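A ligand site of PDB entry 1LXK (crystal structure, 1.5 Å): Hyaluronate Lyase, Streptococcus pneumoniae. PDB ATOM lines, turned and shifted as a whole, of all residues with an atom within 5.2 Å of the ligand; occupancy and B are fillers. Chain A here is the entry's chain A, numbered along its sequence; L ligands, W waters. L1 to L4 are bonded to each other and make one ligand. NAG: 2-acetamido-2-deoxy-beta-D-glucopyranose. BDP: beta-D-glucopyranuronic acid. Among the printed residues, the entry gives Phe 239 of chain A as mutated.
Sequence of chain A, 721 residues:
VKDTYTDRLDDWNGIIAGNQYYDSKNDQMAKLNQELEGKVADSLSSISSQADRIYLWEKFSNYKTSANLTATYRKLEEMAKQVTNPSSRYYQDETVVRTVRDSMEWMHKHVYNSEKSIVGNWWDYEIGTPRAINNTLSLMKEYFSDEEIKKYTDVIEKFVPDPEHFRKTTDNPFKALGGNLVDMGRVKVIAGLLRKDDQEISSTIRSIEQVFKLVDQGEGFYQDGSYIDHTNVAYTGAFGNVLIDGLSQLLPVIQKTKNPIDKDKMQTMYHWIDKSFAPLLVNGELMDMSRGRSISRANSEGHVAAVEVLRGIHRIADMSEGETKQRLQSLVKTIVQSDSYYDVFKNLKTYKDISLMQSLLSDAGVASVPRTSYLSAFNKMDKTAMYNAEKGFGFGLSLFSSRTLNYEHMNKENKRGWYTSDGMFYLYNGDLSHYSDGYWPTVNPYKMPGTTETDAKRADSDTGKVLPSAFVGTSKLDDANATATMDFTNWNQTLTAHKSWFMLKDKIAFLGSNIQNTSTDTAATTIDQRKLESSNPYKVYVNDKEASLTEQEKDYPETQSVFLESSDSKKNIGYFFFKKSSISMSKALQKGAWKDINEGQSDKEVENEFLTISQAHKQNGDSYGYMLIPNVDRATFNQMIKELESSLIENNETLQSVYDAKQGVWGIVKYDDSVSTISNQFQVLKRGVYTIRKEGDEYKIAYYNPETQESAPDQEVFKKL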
ATOM      1  N   ARG A  74     -27.449  25.537  -6.545  1.00  0.00           N
ATOM      2  CA  ARG A  74     -27.441  26.731  -7.402  1.00  0.00           C
ATOM      3  C   ARG A  74     -27.766  27.961  -6.563  1.00  0.00           C
ATOM      4  O   ARG A  74     -27.349  29.077  -6.880  1.00  0.00           O
ATOM      5  CB  ARG A  74     -28.460  26.581  -8.545  1.00  0.00           C
ATOM      6  CG  ARG A  74     -27.821  26.267  -9.890  1.00  0.00           C
ATOM      7  CD  ARG A  74     -28.636  25.263 -10.696  1.00  0.00           C
ATOM      8  NE  ARG A  74     -27.907  24.771 -11.873  1.00  0.00           N
ATOM      9  CZ  ARG A  74     -28.483  24.250 -12.958  1.00  0.00           C
ATOM     10  NH1 ARG A  74     -27.732  23.832 -13.966  1.00  0.00           N
ATOM     11  NH2 ARG A  74     -29.797  24.155 -13.039  1.00  0.00           N
ATOM     12  N   ASN A 121     -32.339  11.622 -11.864  1.00  0.00           N
ATOM     13  CA  ASN A 121     -31.528  11.880 -13.046  1.00  0.00           C
ATOM     14  C   ASN A 121     -30.030  11.874 -12.715  1.00  0.00           C
ATOM     15  O   ASN A 121     -29.581  12.556 -11.795  1.00  0.00           O
ATOM     16  CB  ASN A 121     -31.913  13.228 -13.671  1.00  0.00           C
ATOM     17  CG  ASN A 121     -31.558  13.313 -15.135  1.00  0.00           C
ATOM     18  OD1 ASN A 121     -31.000  12.367 -15.706  1.00  0.00           O
ATOM     19  ND2 ASN A 121     -31.862  14.441 -15.751  1.00  0.00           N
ATOM     20  N   TRP A 122     -29.266  11.095 -13.480  1.00  0.00           N
ATOM     21  CA  TRP A 122     -27.815  11.021 -13.301  1.00  0.00           C
ATOM     22  C   TRP A 122     -27.222  12.414 -13.551  1.00  0.00           C
ATOM     23  O   TRP A 122     -26.244  12.817 -12.917  1.00  0.00           O
ATOM     24  CB  TRP A 122     -27.214  10.033 -14.307  1.00  0.00           C
ATOM     25  CG  TRP A 122     -27.360  10.490 -15.758  1.00  0.00           C
ATOM     26  CD1 TRP A 122     -28.414  10.255 -16.598  1.00  0.00           C
ATOM     27  CD2 TRP A 122     -26.450  11.336 -16.490  1.00  0.00           C
ATOM     28  NE1 TRP A 122     -28.232  10.905 -17.798  1.00  0.00           N
ATOM     29  CE2 TRP A 122     -27.034  11.575 -17.757  1.00  0.00           C
ATOM     30  CE3 TRP A 122     -25.204  11.913 -16.198  1.00  0.00           C
ATOM     31  CZ2 TRP A 122     -26.410  12.371 -18.739  1.00  0.00           C
ATOM     32  CZ3 TRP A 122     -24.585  12.712 -17.172  1.00  0.00           C
ATOM     33  CH2 TRP A 122     -25.190  12.926 -18.421  1.00  0.00           C
ATOM     34  N   TRP A 123     -27.845  13.126 -14.483  1.00  0.00           N
ATOM     35  CA  TRP A 123     -27.424  14.454 -14.898  1.00  0.00           C
ATOM     36  C   TRP A 123     -27.110  15.393 -13.733  1.00  0.00           C
ATOM     37  O   TRP A 123     -26.098  16.091 -13.743  1.00  0.00           O
ATOM     38  CB  TRP A 123     -28.491  15.083 -15.803  1.00  0.00           C
ATOM     39  CG  TRP A 123     -27.995  16.280 -16.505  1.00  0.00           C
ATOM     40  CD1 TRP A 123     -27.348  16.323 -17.712  1.00  0.00           C
ATOM     41  CD2 TRP A 123     -28.070  17.636 -16.043  1.00  0.00           C
ATOM     42  NE1 TRP A 123     -27.019  17.622 -18.020  1.00  0.00           N
ATOM     43  CE2 TRP A 123     -27.456  18.447 -17.012  1.00  0.00           C
ATOM     44  CE3 TRP A 123     -28.595  18.247 -14.883  1.00  0.00           C
ATOM     45  CZ2 TRP A 123     -27.352  19.843 -16.878  1.00  0.00           C
ATOM     46  CZ3 TRP A 123     -28.501  19.623 -14.749  1.00  0.00           C
ATOM     47  CH2 TRP A 123     -27.872  20.407 -15.737  1.00  0.00           C
ATOM     48  N   ASP A 124     -27.981  15.394 -12.723  1.00  0.00           N
ATOM     49  CA  ASP A 124     -27.784  16.244 -11.565  1.00  0.00           C
ATOM     50  C   ASP A 124     -26.598  15.778 -10.725  1.00  0.00           C
ATOM     51  O   ASP A 124     -25.851  16.588 -10.162  1.00  0.00           O
ATOM     52  CB  ASP A 124     -29.055  16.249 -10.701  1.00  0.00           C
ATOM     53  CG  ASP A 124     -30.234  16.881 -11.421  1.00  0.00           C
ATOM     54  OD1 ASP A 124     -30.182  18.099 -11.699  1.00  0.00           O
ATOM     55  OD2 ASP A 124     -31.205  16.147 -11.699  1.00  0.00           O
ATOM     56  N   ARG A 131     -21.287  21.207 -11.066  1.00  0.00           N
ATOM     57  CA  ARG A 131     -20.973  22.513 -11.625  1.00  0.00           C
ATOM     58  C   ARG A 131     -21.264  23.605 -10.595  1.00  0.00           C
ATOM     59  O   ARG A 131     -20.445  24.499 -10.371  1.00  0.00           O
ATOM     60  CB  ARG A 131     -21.791  22.767 -12.886  1.00  0.00           C
ATOM     61  CG  ARG A 131     -21.156  22.187 -14.142  1.00  0.00           C
ATOM     62  CD  ARG A 131     -22.108  22.253 -15.314  1.00  0.00           C
ATOM     63  NE  ARG A 131     -22.679  23.591 -15.463  1.00  0.00           N
ATOM     64  CZ  ARG A 131     -23.836  23.860 -16.060  1.00  0.00           C
ATOM     65  NH1 ARG A 131     -24.564  22.873 -16.582  1.00  0.00           N
ATOM     66  NH2 ARG A 131     -24.274  25.106 -16.137  1.00  0.00           N
ATOM     67  N   ARG A 167     -22.022   8.651 -16.058  1.00  0.00           N
ATOM     68  CA  ARG A 167     -22.755   7.527 -15.484  1.00  0.00           C
ATOM     69  C   ARG A 167     -21.810   6.345 -15.255  1.00  0.00           C
ATOM     70  O   ARG A 167     -22.169   5.192 -15.504  1.00  0.00           O
ATOM     71  CB  ARG A 167     -23.906   7.112 -16.401  1.00  0.00           C
ATOM     72  CG  ARG A 167     -25.158   7.946 -16.200  1.00  0.00           C
ATOM     73  CD  ARG A 167     -26.379   7.225 -16.722  1.00  0.00           C
ATOM     74  NE  ARG A 167     -26.169   6.763 -18.087  1.00  0.00           N
ATOM     75  CZ  ARG A 167     -27.058   6.899 -19.059  1.00  0.00           C
ATOM     76  NH1 ARG A 167     -28.236   7.463 -18.813  1.00  0.00           N
ATOM     77  NH2 ARG A 167     -26.786   6.461 -20.287  1.00  0.00           N
ATOM     78  N   PHE A 174     -21.895   6.066 -20.541  1.00  0.00           N
ATOM     79  CA  PHE A 174     -21.804   6.394 -21.962  1.00  0.00           C
ATOM     80  C   PHE A 174     -20.636   7.331 -22.212  1.00  0.00           C
ATOM     81  O   PHE A 174     -20.181   8.020 -21.301  1.00  0.00           O
ATOM     82  CB  PHE A 174     -23.113   7.006 -22.467  1.00  0.00           C
ATOM     83  CG  PHE A 174     -23.416   8.376 -21.919  1.00  0.00           C
ATOM     84  CD1 PHE A 174     -23.051   9.516 -22.633  1.00  0.00           C
ATOM     85  CD2 PHE A 174     -24.104   8.529 -20.724  1.00  0.00           C
ATOM     86  CE1 PHE A 174     -23.363  10.794 -22.164  1.00  0.00           C
ATOM     87  CE2 PHE A 174     -24.414   9.801 -20.239  1.00  0.00           C
ATOM     88  CZ  PHE A 174     -24.043  10.928 -20.958  1.00  0.00           C
ATOM     89  N   ASN A 180     -22.353  17.295 -23.650  1.00  0.00           N
ATOM     90  CA  ASN A 180     -21.994  16.531 -22.460  1.00  0.00           C
ATOM     91  C   ASN A 180     -20.484  16.556 -22.207  1.00  0.00           C
ATOM     92  O   ASN A 180     -20.040  16.664 -21.067  1.00  0.00           O
ATOM     93  CB  ASN A 180     -22.442  15.081 -22.595  1.00  0.00           C
ATOM     94  CG  ASN A 180     -23.928  14.900 -22.369  1.00  0.00           C
ATOM     95  OD1 ASN A 180     -24.505  13.906 -22.808  1.00  0.00           O
ATOM     96  ND2 ASN A 180     -24.537  15.857 -21.687  1.00  0.00           N
ATOM     97  N   ARG A 186     -16.483  21.498 -17.590  1.00  0.00           N
ATOM     98  CA  ARG A 186     -16.878  22.491 -16.603  1.00  0.00           C
ATOM     99  C   ARG A 186     -17.023  21.816 -15.255  1.00  0.00           C
ATOM    100  O   ARG A 186     -17.183  22.469 -14.215  1.00  0.00           O
ATOM    101  CB  ARG A 186     -18.203  23.148 -17.019  1.00  0.00           C
ATOM    102  CG  ARG A 186     -18.025  24.229 -18.074  1.00  0.00           C
ATOM    103  CD  ARG A 186     -19.191  25.201 -18.081  1.00  0.00           C
ATOM    104  NE  ARG A 186     -20.442  24.527 -18.386  1.00  0.00           N
ATOM    105  CZ  ARG A 186     -21.559  25.156 -18.747  1.00  0.00           C
ATOM    106  NH1 ARG A 186     -21.579  26.491 -18.832  1.00  0.00           N
ATOM    107  NH2 ARG A 186     -22.665  24.468 -18.995  1.00  0.00           N
ATOM    108  N   GLU A 219     -23.301  11.083 -33.091  1.00  0.00           N
ATOM    109  CA  GLU A 219     -23.515  12.408 -32.542  1.00  0.00           C
ATOM    110  C   GLU A 219     -22.352  13.339 -32.855  1.00  0.00           C
ATOM    111  O   GLU A 219     -21.199  12.920 -32.910  1.00  0.00           O
ATOM    112  CB  GLU A 219     -23.714  12.294 -31.035  1.00  0.00           C
ATOM    113  CG  GLU A 219     -24.838  11.348 -30.651  1.00  0.00           C
ATOM    114  CD  GLU A 219     -24.832  10.975 -29.186  1.00  0.00           C
ATOM    115  OE1 GLU A 219     -23.766  11.086 -28.540  1.00  0.00           O
ATOM    116  OE2 GLU A 219     -25.893  10.578 -28.670  1.00  0.00           O
ATOM    117  N   HIS A 230     -28.119  12.740 -28.899  1.00  0.00           N
ATOM    118  CA  HIS A 230     -29.024  11.724 -28.378  1.00  0.00           C
ATOM    119  C   HIS A 230     -29.306  10.699 -29.469  1.00  0.00           C
ATOM    120  O   HIS A 230     -30.448  10.464 -29.853  1.00  0.00           O
ATOM    121  CB  HIS A 230     -30.296  12.368 -27.844  1.00  0.00           C
ATOM    122  CG  HIS A 230     -30.178  12.845 -26.428  1.00  0.00           C
ATOM    123  ND1 HIS A 230     -31.255  13.256 -25.674  1.00  0.00           N
ATOM    124  CD2 HIS A 230     -29.084  12.973 -25.629  1.00  0.00           C
ATOM    125  CE1 HIS A 230     -30.847  13.610 -24.470  1.00  0.00           C
ATOM    126  NE2 HIS A 230     -29.528  13.457 -24.424  1.00  0.00           N
ATOM    127  N   ALA A 238     -30.083  23.111 -28.907  1.00  0.00           N
ATOM    128  CA  ALA A 238     -30.223  22.914 -27.472  1.00  0.00           C
ATOM    129  C   ALA A 238     -28.888  22.388 -26.950  1.00  0.00           C
ATOM    130  O   ALA A 238     -28.248  23.009 -26.103  1.00  0.00           O
ATOM    131  CB  ALA A 238     -31.355  21.949 -27.163  1.00  0.00           C
ATOM    132  N   PHE A 239     -28.472  21.236 -27.470  1.00  0.00           N
ATOM    133  CA  PHE A 239     -27.198  20.662 -27.065  1.00  0.00           C
ATOM    134  C   PHE A 239     -26.063  21.418 -27.737  1.00  0.00           C
ATOM    135  O   PHE A 239     -24.971  21.558 -27.171  1.00  0.00           O
ATOM    136  CB  PHE A 239     -27.156  19.176 -27.436  1.00  0.00           C
ATOM    137  CG  PHE A 239     -27.881  18.303 -26.451  1.00  0.00           C
ATOM    138  CD1 PHE A 239     -29.233  18.026 -26.605  1.00  0.00           C
ATOM    139  CD2 PHE A 239     -27.216  17.789 -25.347  1.00  0.00           C
ATOM    140  CE1 PHE A 239     -29.916  17.248 -25.683  1.00  0.00           C
ATOM    141  CE2 PHE A 239     -27.891  17.003 -24.417  1.00  0.00           C
ATOM    142  CZ  PHE A 239     -29.237  16.733 -24.581  1.00  0.00           C
ATOM    143  N   VAL A 242     -25.466  24.389 -25.430  1.00  0.00           N
ATOM    144  CA  VAL A 242     -24.667  24.029 -24.265  1.00  0.00           C
ATOM    145  C   VAL A 242     -23.213  23.861 -24.687  1.00  0.00           C
ATOM    146  O   VAL A 242     -22.308  24.320 -24.008  1.00  0.00           O
ATOM    147  CB  VAL A 242     -25.202  22.738 -23.614  1.00  0.00           C
ATOM    148  CG1 VAL A 242     -24.238  22.250 -22.546  1.00  0.00           C
ATOM    149  CG2 VAL A 242     -26.589  22.980 -23.016  1.00  0.00           C
ATOM    150  N   ASP A 245     -21.781  27.384 -25.561  1.00  0.00           N
ATOM    151  CA  ASP A 245     -21.900  28.206 -24.379  1.00  0.00           C
ATOM    152  C   ASP A 245     -20.813  27.821 -23.368  1.00  0.00           C
ATOM    153  O   ASP A 245     -20.009  28.653 -22.948  1.00  0.00           O
ATOM    154  CB  ASP A 245     -23.300  28.016 -23.774  1.00  0.00           C
ATOM    155  CG  ASP A 245     -23.636  29.054 -22.721  1.00  0.00           C
ATOM    156  OD1 ASP A 245     -23.003  30.127 -22.721  1.00  0.00           O
ATOM    157  OD2 ASP A 245     -24.537  28.782 -21.889  1.00  0.00           O
ATOM    158  N   ARG A 293     -36.569  19.020 -27.415  1.00  0.00           N
ATOM    159  CA  ARG A 293     -37.576  19.175 -26.358  1.00  0.00           C
ATOM    160  C   ARG A 293     -37.528  20.492 -25.584  1.00  0.00           C
ATOM    161  O   ARG A 293     -38.415  20.771 -24.782  1.00  0.00           O
ATOM    162  CB  ARG A 293     -37.502  17.990 -25.371  1.00  0.00           C
ATOM    163  CG  ARG A 293     -36.354  18.050 -24.387  1.00  0.00           C
ATOM    164  CD  ARG A 293     -36.132  16.696 -23.699  1.00  0.00           C
ATOM    165  NE  ARG A 293     -35.382  16.849 -22.445  1.00  0.00           N
ATOM    166  CZ  ARG A 293     -34.098  16.537 -22.300  1.00  0.00           C
ATOM    167  NH1 ARG A 293     -33.389  16.050 -23.304  1.00  0.00           N
ATOM    168  NH2 ARG A 293     -33.508  16.740 -21.124  1.00  0.00           N
ATOM    169  N   SER A 294     -36.497  21.301 -25.841  1.00  0.00           N
ATOM    170  CA  SER A 294     -36.349  22.594 -25.178  1.00  0.00           C
ATOM    171  C   SER A 294     -37.501  23.543 -25.508  1.00  0.00           C
ATOM    172  O   SER A 294     -37.786  24.467 -24.763  1.00  0.00           O
ATOM    173  CB  SER A 294     -35.043  23.261 -25.601  1.00  0.00           C
ATOM    174  OG  SER A 294     -33.966  22.734 -24.858  1.00  0.00           O
ATOM    175  N   ARG A 297     -40.096  24.433 -22.957  1.00  0.00           N
ATOM    176  CA  ARG A 297     -39.700  25.172 -21.750  1.00  0.00           C
ATOM    177  C   ARG A 297     -40.111  26.639 -21.926  1.00  0.00           C
ATOM    178  O   ARG A 297     -39.675  27.299 -22.874  1.00  0.00           O
ATOM    179  CB  ARG A 297     -38.181  25.081 -21.544  1.00  0.00           C
ATOM    180  CG  ARG A 297     -37.726  23.679 -21.231  1.00  0.00           C
ATOM    181  CD  ARG A 297     -36.216  23.555 -21.311  1.00  0.00           C
ATOM    182  NE  ARG A 297     -35.804  22.171 -21.134  1.00  0.00           N
ATOM    183  CZ  ARG A 297     -34.582  21.716 -21.394  1.00  0.00           C
ATOM    184  NH1 ARG A 297     -33.648  22.549 -21.853  1.00  0.00           N
ATOM    185  NH2 ARG A 297     -34.304  20.433 -21.217  1.00  0.00           N
ATOM    186  N   GLU A 308     -28.122  32.296 -25.945  1.00  0.00           N
ATOM    187  CA  GLU A 308     -27.202  31.295 -25.386  1.00  0.00           C
ATOM    188  C   GLU A 308     -26.074  31.098 -26.382  1.00  0.00           C
ATOM    189  O   GLU A 308     -24.903  31.005 -26.018  1.00  0.00           O
ATOM    190  CB  GLU A 308     -27.909  29.952 -25.244  1.00  0.00           C
ATOM    191  CG  GLU A 308     -28.515  29.681 -23.914  1.00  0.00           C
ATOM    192  CD  GLU A 308     -28.929  28.239 -23.813  1.00  0.00           C
ATOM    193  OE1 GLU A 308     -29.739  27.784 -24.653  1.00  0.00           O
ATOM    194  OE2 GLU A 308     -28.419  27.536 -22.914  1.00  0.00           O
ATOM    195  N   ARG A 311     -24.021  34.631 -27.048  1.00  0.00           N
ATOM    196  CA  ARG A 311     -23.052  34.964 -26.008  1.00  0.00           C
ATOM    197  C   ARG A 311     -21.835  34.060 -26.125  1.00  0.00           C
ATOM    198  O   ARG A 311     -20.718  34.455 -25.768  1.00  0.00           O
ATOM    199  CB  ARG A 311     -23.685  34.841 -24.628  1.00  0.00           C
ATOM    200  CG  ARG A 311     -24.185  33.462 -24.266  1.00  0.00           C
ATOM    201  CD  ARG A 311     -25.113  33.542 -23.042  1.00  0.00           C
ATOM    202  NE  ARG A 311     -25.193  32.268 -22.351  1.00  0.00           N
ATOM    203  CZ  ARG A 311     -26.083  31.973 -21.405  1.00  0.00           C
ATOM    204  NH1 ARG A 311     -26.983  32.883 -21.040  1.00  0.00           N
ATOM    205  NH2 ARG A 311     -26.075  30.785 -20.842  1.00  0.00           N
ATOM    206  N   MET A 410     -38.650  13.391 -23.645  1.00  0.00           N
ATOM    207  CA  MET A 410     -37.833  12.770 -22.603  1.00  0.00           C
ATOM    208  C   MET A 410     -38.011  13.568 -21.328  1.00  0.00           C
ATOM    209  O   MET A 410     -38.209  14.777 -21.377  1.00  0.00           O
ATOM    210  CB  MET A 410     -36.365  12.772 -23.041  1.00  0.00           C
ATOM    211  CG  MET A 410     -35.414  12.004 -22.138  1.00  0.00           C
ATOM    212  SD  MET A 410     -33.681  12.346 -22.527  1.00  0.00           S
ATOM    213  CE  MET A 410     -33.468  11.290 -23.952  1.00  0.00           C
ATOM    214  N   ASN A 411     -37.927  12.876 -20.192  1.00  0.00           N
ATOM    215  CA  ASN A 411     -38.072  13.516 -18.884  1.00  0.00           C
ATOM    216  C   ASN A 411     -39.352  14.315 -18.744  1.00  0.00           C
ATOM    217  O   ASN A 411     -39.386  15.343 -18.067  1.00  0.00           O
ATOM    218  CB  ASN A 411     -36.872  14.435 -18.601  1.00  0.00           C
ATOM    219  CG  ASN A 411     -35.552  13.693 -18.630  1.00  0.00           C
ATOM    220  OD1 ASN A 411     -35.409  12.615 -18.054  1.00  0.00           O
ATOM    221  ND2 ASN A 411     -34.570  14.283 -19.298  1.00  0.00           N
HETATM  222  C1  NAG L   1     -30.112   8.167 -22.294  1.00  0.00           C
HETATM  223  C2  NAG L   1     -30.238   9.019 -20.998  1.00  0.00           C
HETATM  224  C3  NAG L   1     -29.752  10.462 -21.314  1.00  0.00           C
HETATM  225  C4  NAG L   1     -28.240  10.391 -21.787  1.00  0.00           C
HETATM  226  C5  NAG L   1     -28.155   9.499 -23.086  1.00  0.00           C
HETATM  227  C6  NAG L   1     -26.718   9.345 -23.613  1.00  0.00           C
HETATM  228  C7  NAG L   1     -32.040   9.037 -19.164  1.00  0.00           C
HETATM  229  C8  NAG L   1     -33.535   9.053 -18.978  1.00  0.00           C
HETATM  230  N2  NAG L   1     -31.677   9.032 -20.533  1.00  0.00           N
HETATM  231  O1  NAG L   1     -30.534   6.844 -22.057  1.00  0.00           O
HETATM  232  O3  NAG L   1     -29.854  11.297 -20.123  1.00  0.00           O
HETATM  233  O4  NAG L   1     -27.738  11.719 -22.107  1.00  0.00           O
HETATM  234  O5  NAG L   1     -28.670   8.119 -22.810  1.00  0.00           O
HETATM  235  O6  NAG L   1     -26.607   9.688 -25.011  1.00  0.00           O
HETATM  236  O7  NAG L   1     -31.251   9.016 -18.208  1.00  0.00           O
HETATM  237  C1  BDP L   2     -30.331  12.593 -20.331  1.00  0.00           C
HETATM  238  C2  BDP L   2     -31.022  13.213 -19.089  1.00  0.00           C
HETATM  239  C3  BDP L   2     -31.491  14.634 -19.494  1.00  0.00           C
HETATM  240  C4  BDP L   2     -30.237  15.466 -19.852  1.00  0.00           C
HETATM  241  C5  BDP L   2     -29.223  14.973 -21.093  1.00  0.00           C
HETATM  242  C6  BDP L   2     -28.173  15.504 -21.455  1.00  0.00           C
HETATM  243  O2  BDP L   2     -32.172  12.398 -18.726  1.00  0.00           O
HETATM  244  O3  BDP L   2     -32.168  15.251 -18.380  1.00  0.00           O
HETATM  245  O4  BDP L   2     -30.609  16.813 -20.280  1.00  0.00           O
HETATM  246  O5  BDP L   2     -29.183  13.396 -20.743  1.00  0.00           O
HETATM  247  O6A BDP L   2     -27.942  16.677 -21.038  1.00  0.00           O
HETATM  248  O6B BDP L   2     -27.439  14.787 -22.184  1.00  0.00           O
HETATM  249  C1  NAG L   3     -30.435  17.923 -19.442  1.00  0.00           C
HETATM  250  C2  NAG L   3     -30.893  19.234 -20.185  1.00  0.00           C
HETATM  251  C3  NAG L   3     -30.683  20.433 -19.235  1.00  0.00           C
HETATM  252  C4  NAG L   3     -31.551  20.243 -17.963  1.00  0.00           C
HETATM  253  C5  NAG L   3     -31.089  18.916 -17.239  1.00  0.00           C
HETATM  254  C6  NAG L   3     -31.922  18.642 -15.968  1.00  0.00           C
HETATM  255  C7  NAG L   3     -30.652  19.956 -22.639  1.00  0.00           C
HETATM  256  C8  NAG L   3     -29.640  20.124 -23.726  1.00  0.00           C
HETATM  257  N2  NAG L   3     -30.072  19.449 -21.446  1.00  0.00           N
HETATM  258  O3  NAG L   3     -31.090  21.644 -19.911  1.00  0.00           O
HETATM  259  O4  NAG L   3     -31.369  21.362 -17.047  1.00  0.00           O
HETATM  260  O5  NAG L   3     -31.254  17.745 -18.153  1.00  0.00           O
HETATM  261  O6  NAG L   3     -33.318  18.427 -16.248  1.00  0.00           O
HETATM  262  O7  NAG L   3     -31.831  20.259 -22.795  1.00  0.00           O
HETATM  263  C1  BDP L   4     -30.101  22.612 -20.081  1.00  0.00           C
HETATM  264  C2  BDP L   4     -30.654  23.819 -20.809  1.00  0.00           C
HETATM  265  C3  BDP L   4     -29.461  24.824 -20.909  1.00  0.00           C
HETATM  266  C4  BDP L   4     -28.960  25.185 -19.503  1.00  0.00           C
HETATM  267  C5  BDP L   4     -28.506  24.066 -18.859  1.00  0.00           C
HETATM  268  C6  BDP L   4     -28.016  24.323 -17.454  1.00  0.00           C
HETATM  269  O2  BDP L   4     -31.183  23.399 -22.091  1.00  0.00           O
HETATM  270  O3  BDP L   4     -29.956  25.993 -21.609  1.00  0.00           O
HETATM  271  O4  BDP L   4     -27.835  26.165 -19.479  1.00  0.00           O
HETATM  272  O5  BDP L   4     -29.542  23.014 -18.822  1.00  0.00           O
HETATM  273  O6A BDP L   4     -26.810  24.660 -17.382  1.00  0.00           O
HETATM  274  O6B BDP L   4     -28.866  24.150 -16.553  1.00  0.00           O
HETATM  275  O   HOH W   1     -26.843  27.683 -17.265  1.00  0.00           O
HETATM  276  O   HOH W   2     -30.660   7.024 -16.638  1.00  0.00           O
HETATM  277  O   HOH W   3     -25.473  18.424 -20.016  1.00  0.00           O
HETATM  278  O   HOH W   4     -28.463  28.894 -18.711  1.00  0.00           O
HETATM  279  O   HOH W   5     -27.545  20.164 -20.364  1.00  0.00           O
HETATM  280  O   HOH W   6     -29.142   8.480 -26.481  1.00  0.00           O
HETATM  281  O   HOH W   7     -32.586   6.568 -24.650  1.00  0.00           O
HETATM  282  O   HOH W   8     -34.270  18.658 -13.699  1.00  0.00           O
HETATM  283  O   HOH W   9     -33.457  19.850 -25.096  1.00  0.00           O
HETATM  284  O   HOH W  10     -31.255  22.034 -14.255  1.00  0.00           O
HETATM  285  O   HOH W  11     -30.961   6.003 -19.143  1.00  0.00           O
HETATM  286  O   HOH W  12     -33.551  25.379 -22.292  1.00  0.00           O
HETATM  287  O   HOH W  13     -25.369  24.674 -19.999  1.00  0.00           O
HETATM  288  O   HOH W  14     -29.991  24.087 -24.279  1.00  0.00           O
HETATM  289  O   HOH W  15     -34.206  17.585 -18.667  1.00  0.00           O
HETATM  290  O   HOH W  16     -26.063  26.436 -22.077  1.00  0.00           O
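An oxygen (O3) of BDP L4 sits at hydrogen-bond distance from the side-chain carboxylate (OE2) of Glu 308 (2.5 Å).
The guanidinium group (NH1) of Arg 297 is in hydrogen-bond range of an oxygen (O2) of BDP L4, 2.6 Å away.
The side-chain amide nitrogen (ND2) of Asn 411 sits at hydrogen-bond distance from an oxygen (O3) of BDP L2 (2.7 Å).
An oxygen (O3) of BDP L2 is in hydrogen-bond range of the side-chain amide nitrogen (ND2) of Asn 121 (2.8 Å).
An oxygen (O6B) of BDP L4 lies within salt-bridge range of the guanidinium group (NH1) of Arg 74 (2.8 Å).
NH2 of Arg 131 is in salt-bridge range of O6A of BDP L4, 2.9 Å away.
An oxygen (O3) of NAG L1 lies within hydrogen-bond range of the indole nitrogen (NE1) of Trp 122, 2.9 Å away.
The guanidinium group (NH2) of Arg 293 is in hydrogen-bond range of an oxygen (O4) of BDP L2 (3.0 Å).
An oxygen (O6B) of BDP L2 sits close to the side-chain amide oxygen (OD1) of Asn 180, 3.1 Å away.
The indole nitrogen of Trp 123 lies within hydrogen-bond range of an oxygen (O6A) of BDP L2 (3.3 Å).
An oxygen (O6B) of BDP L2 lies within hydrogen-bond range of a ring nitrogen (NE2) of His 230.
An oxygen (O7) of NAG L1 lies close to the guanidinium group (NH1) of Arg 167, 3.4 Å away.
OG of Ser 294 lies within hydrogen-bond range of NH1 of Arg 297.
The guanidinium group (NH2) of Arg 293 sits close to the side-chain amide nitrogen (ND2) of Asn 411.
The side-chain amide oxygen of Asn 121 lies close to the backbone NH of Trp 123.
The side-chain sulfur (SD) of Met 410 lies within hydrogen-bond range of the guanidinium group (NH1) of Arg 293.
The side-chain carboxylate (OE2) of Glu 219 is in hydrogen-bond range of the backbone NH (N) of His 230 (3.1 Å).
CD1 of Phe 174 touches C6 of NAG L1, 3.8 Å away.
OE2 of Glu 219 touches O6 of NAG L1, at 3.8 Å.
Ala 238 touches the ligand.
CE2 of Phe 239 touches O6B of BDP L2, 3.2 Å away.
OG of Ser 294 touches O7 of NAG L3 (3.9 Å).
The nearest printed residue that does not touch the ligand is Val 242 (4.01 Å).
Water W14 bridges O2 of BDP L4 (2.6 Å) and O of Ala 238 (2.7 Å).
Water W2 bridges an oxygen (O7) of NAG L1 (2.6 Å) and the guanidinium group of Arg 167 (3.3 Å).
Water W5 bridges a nitrogen (N2) of NAG L3 and the indole nitrogen of Trp 123.
Water W13 bridges the guanidinium group of Arg 186 (2.9 Å) and an oxygen (O4) of BDP L4 (2.9 Å).
Water W11 bridges an oxygen (O1) of NAG L1 (3.1 Å) and the guanidinium group of Arg 167 (3.1 Å).
Water W16 lies within hydrogen-bond range of the side-chain carboxylate of Glu 308, the side-chain carboxylate of Asp 245 and an oxygen (O4) of BDP L4.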
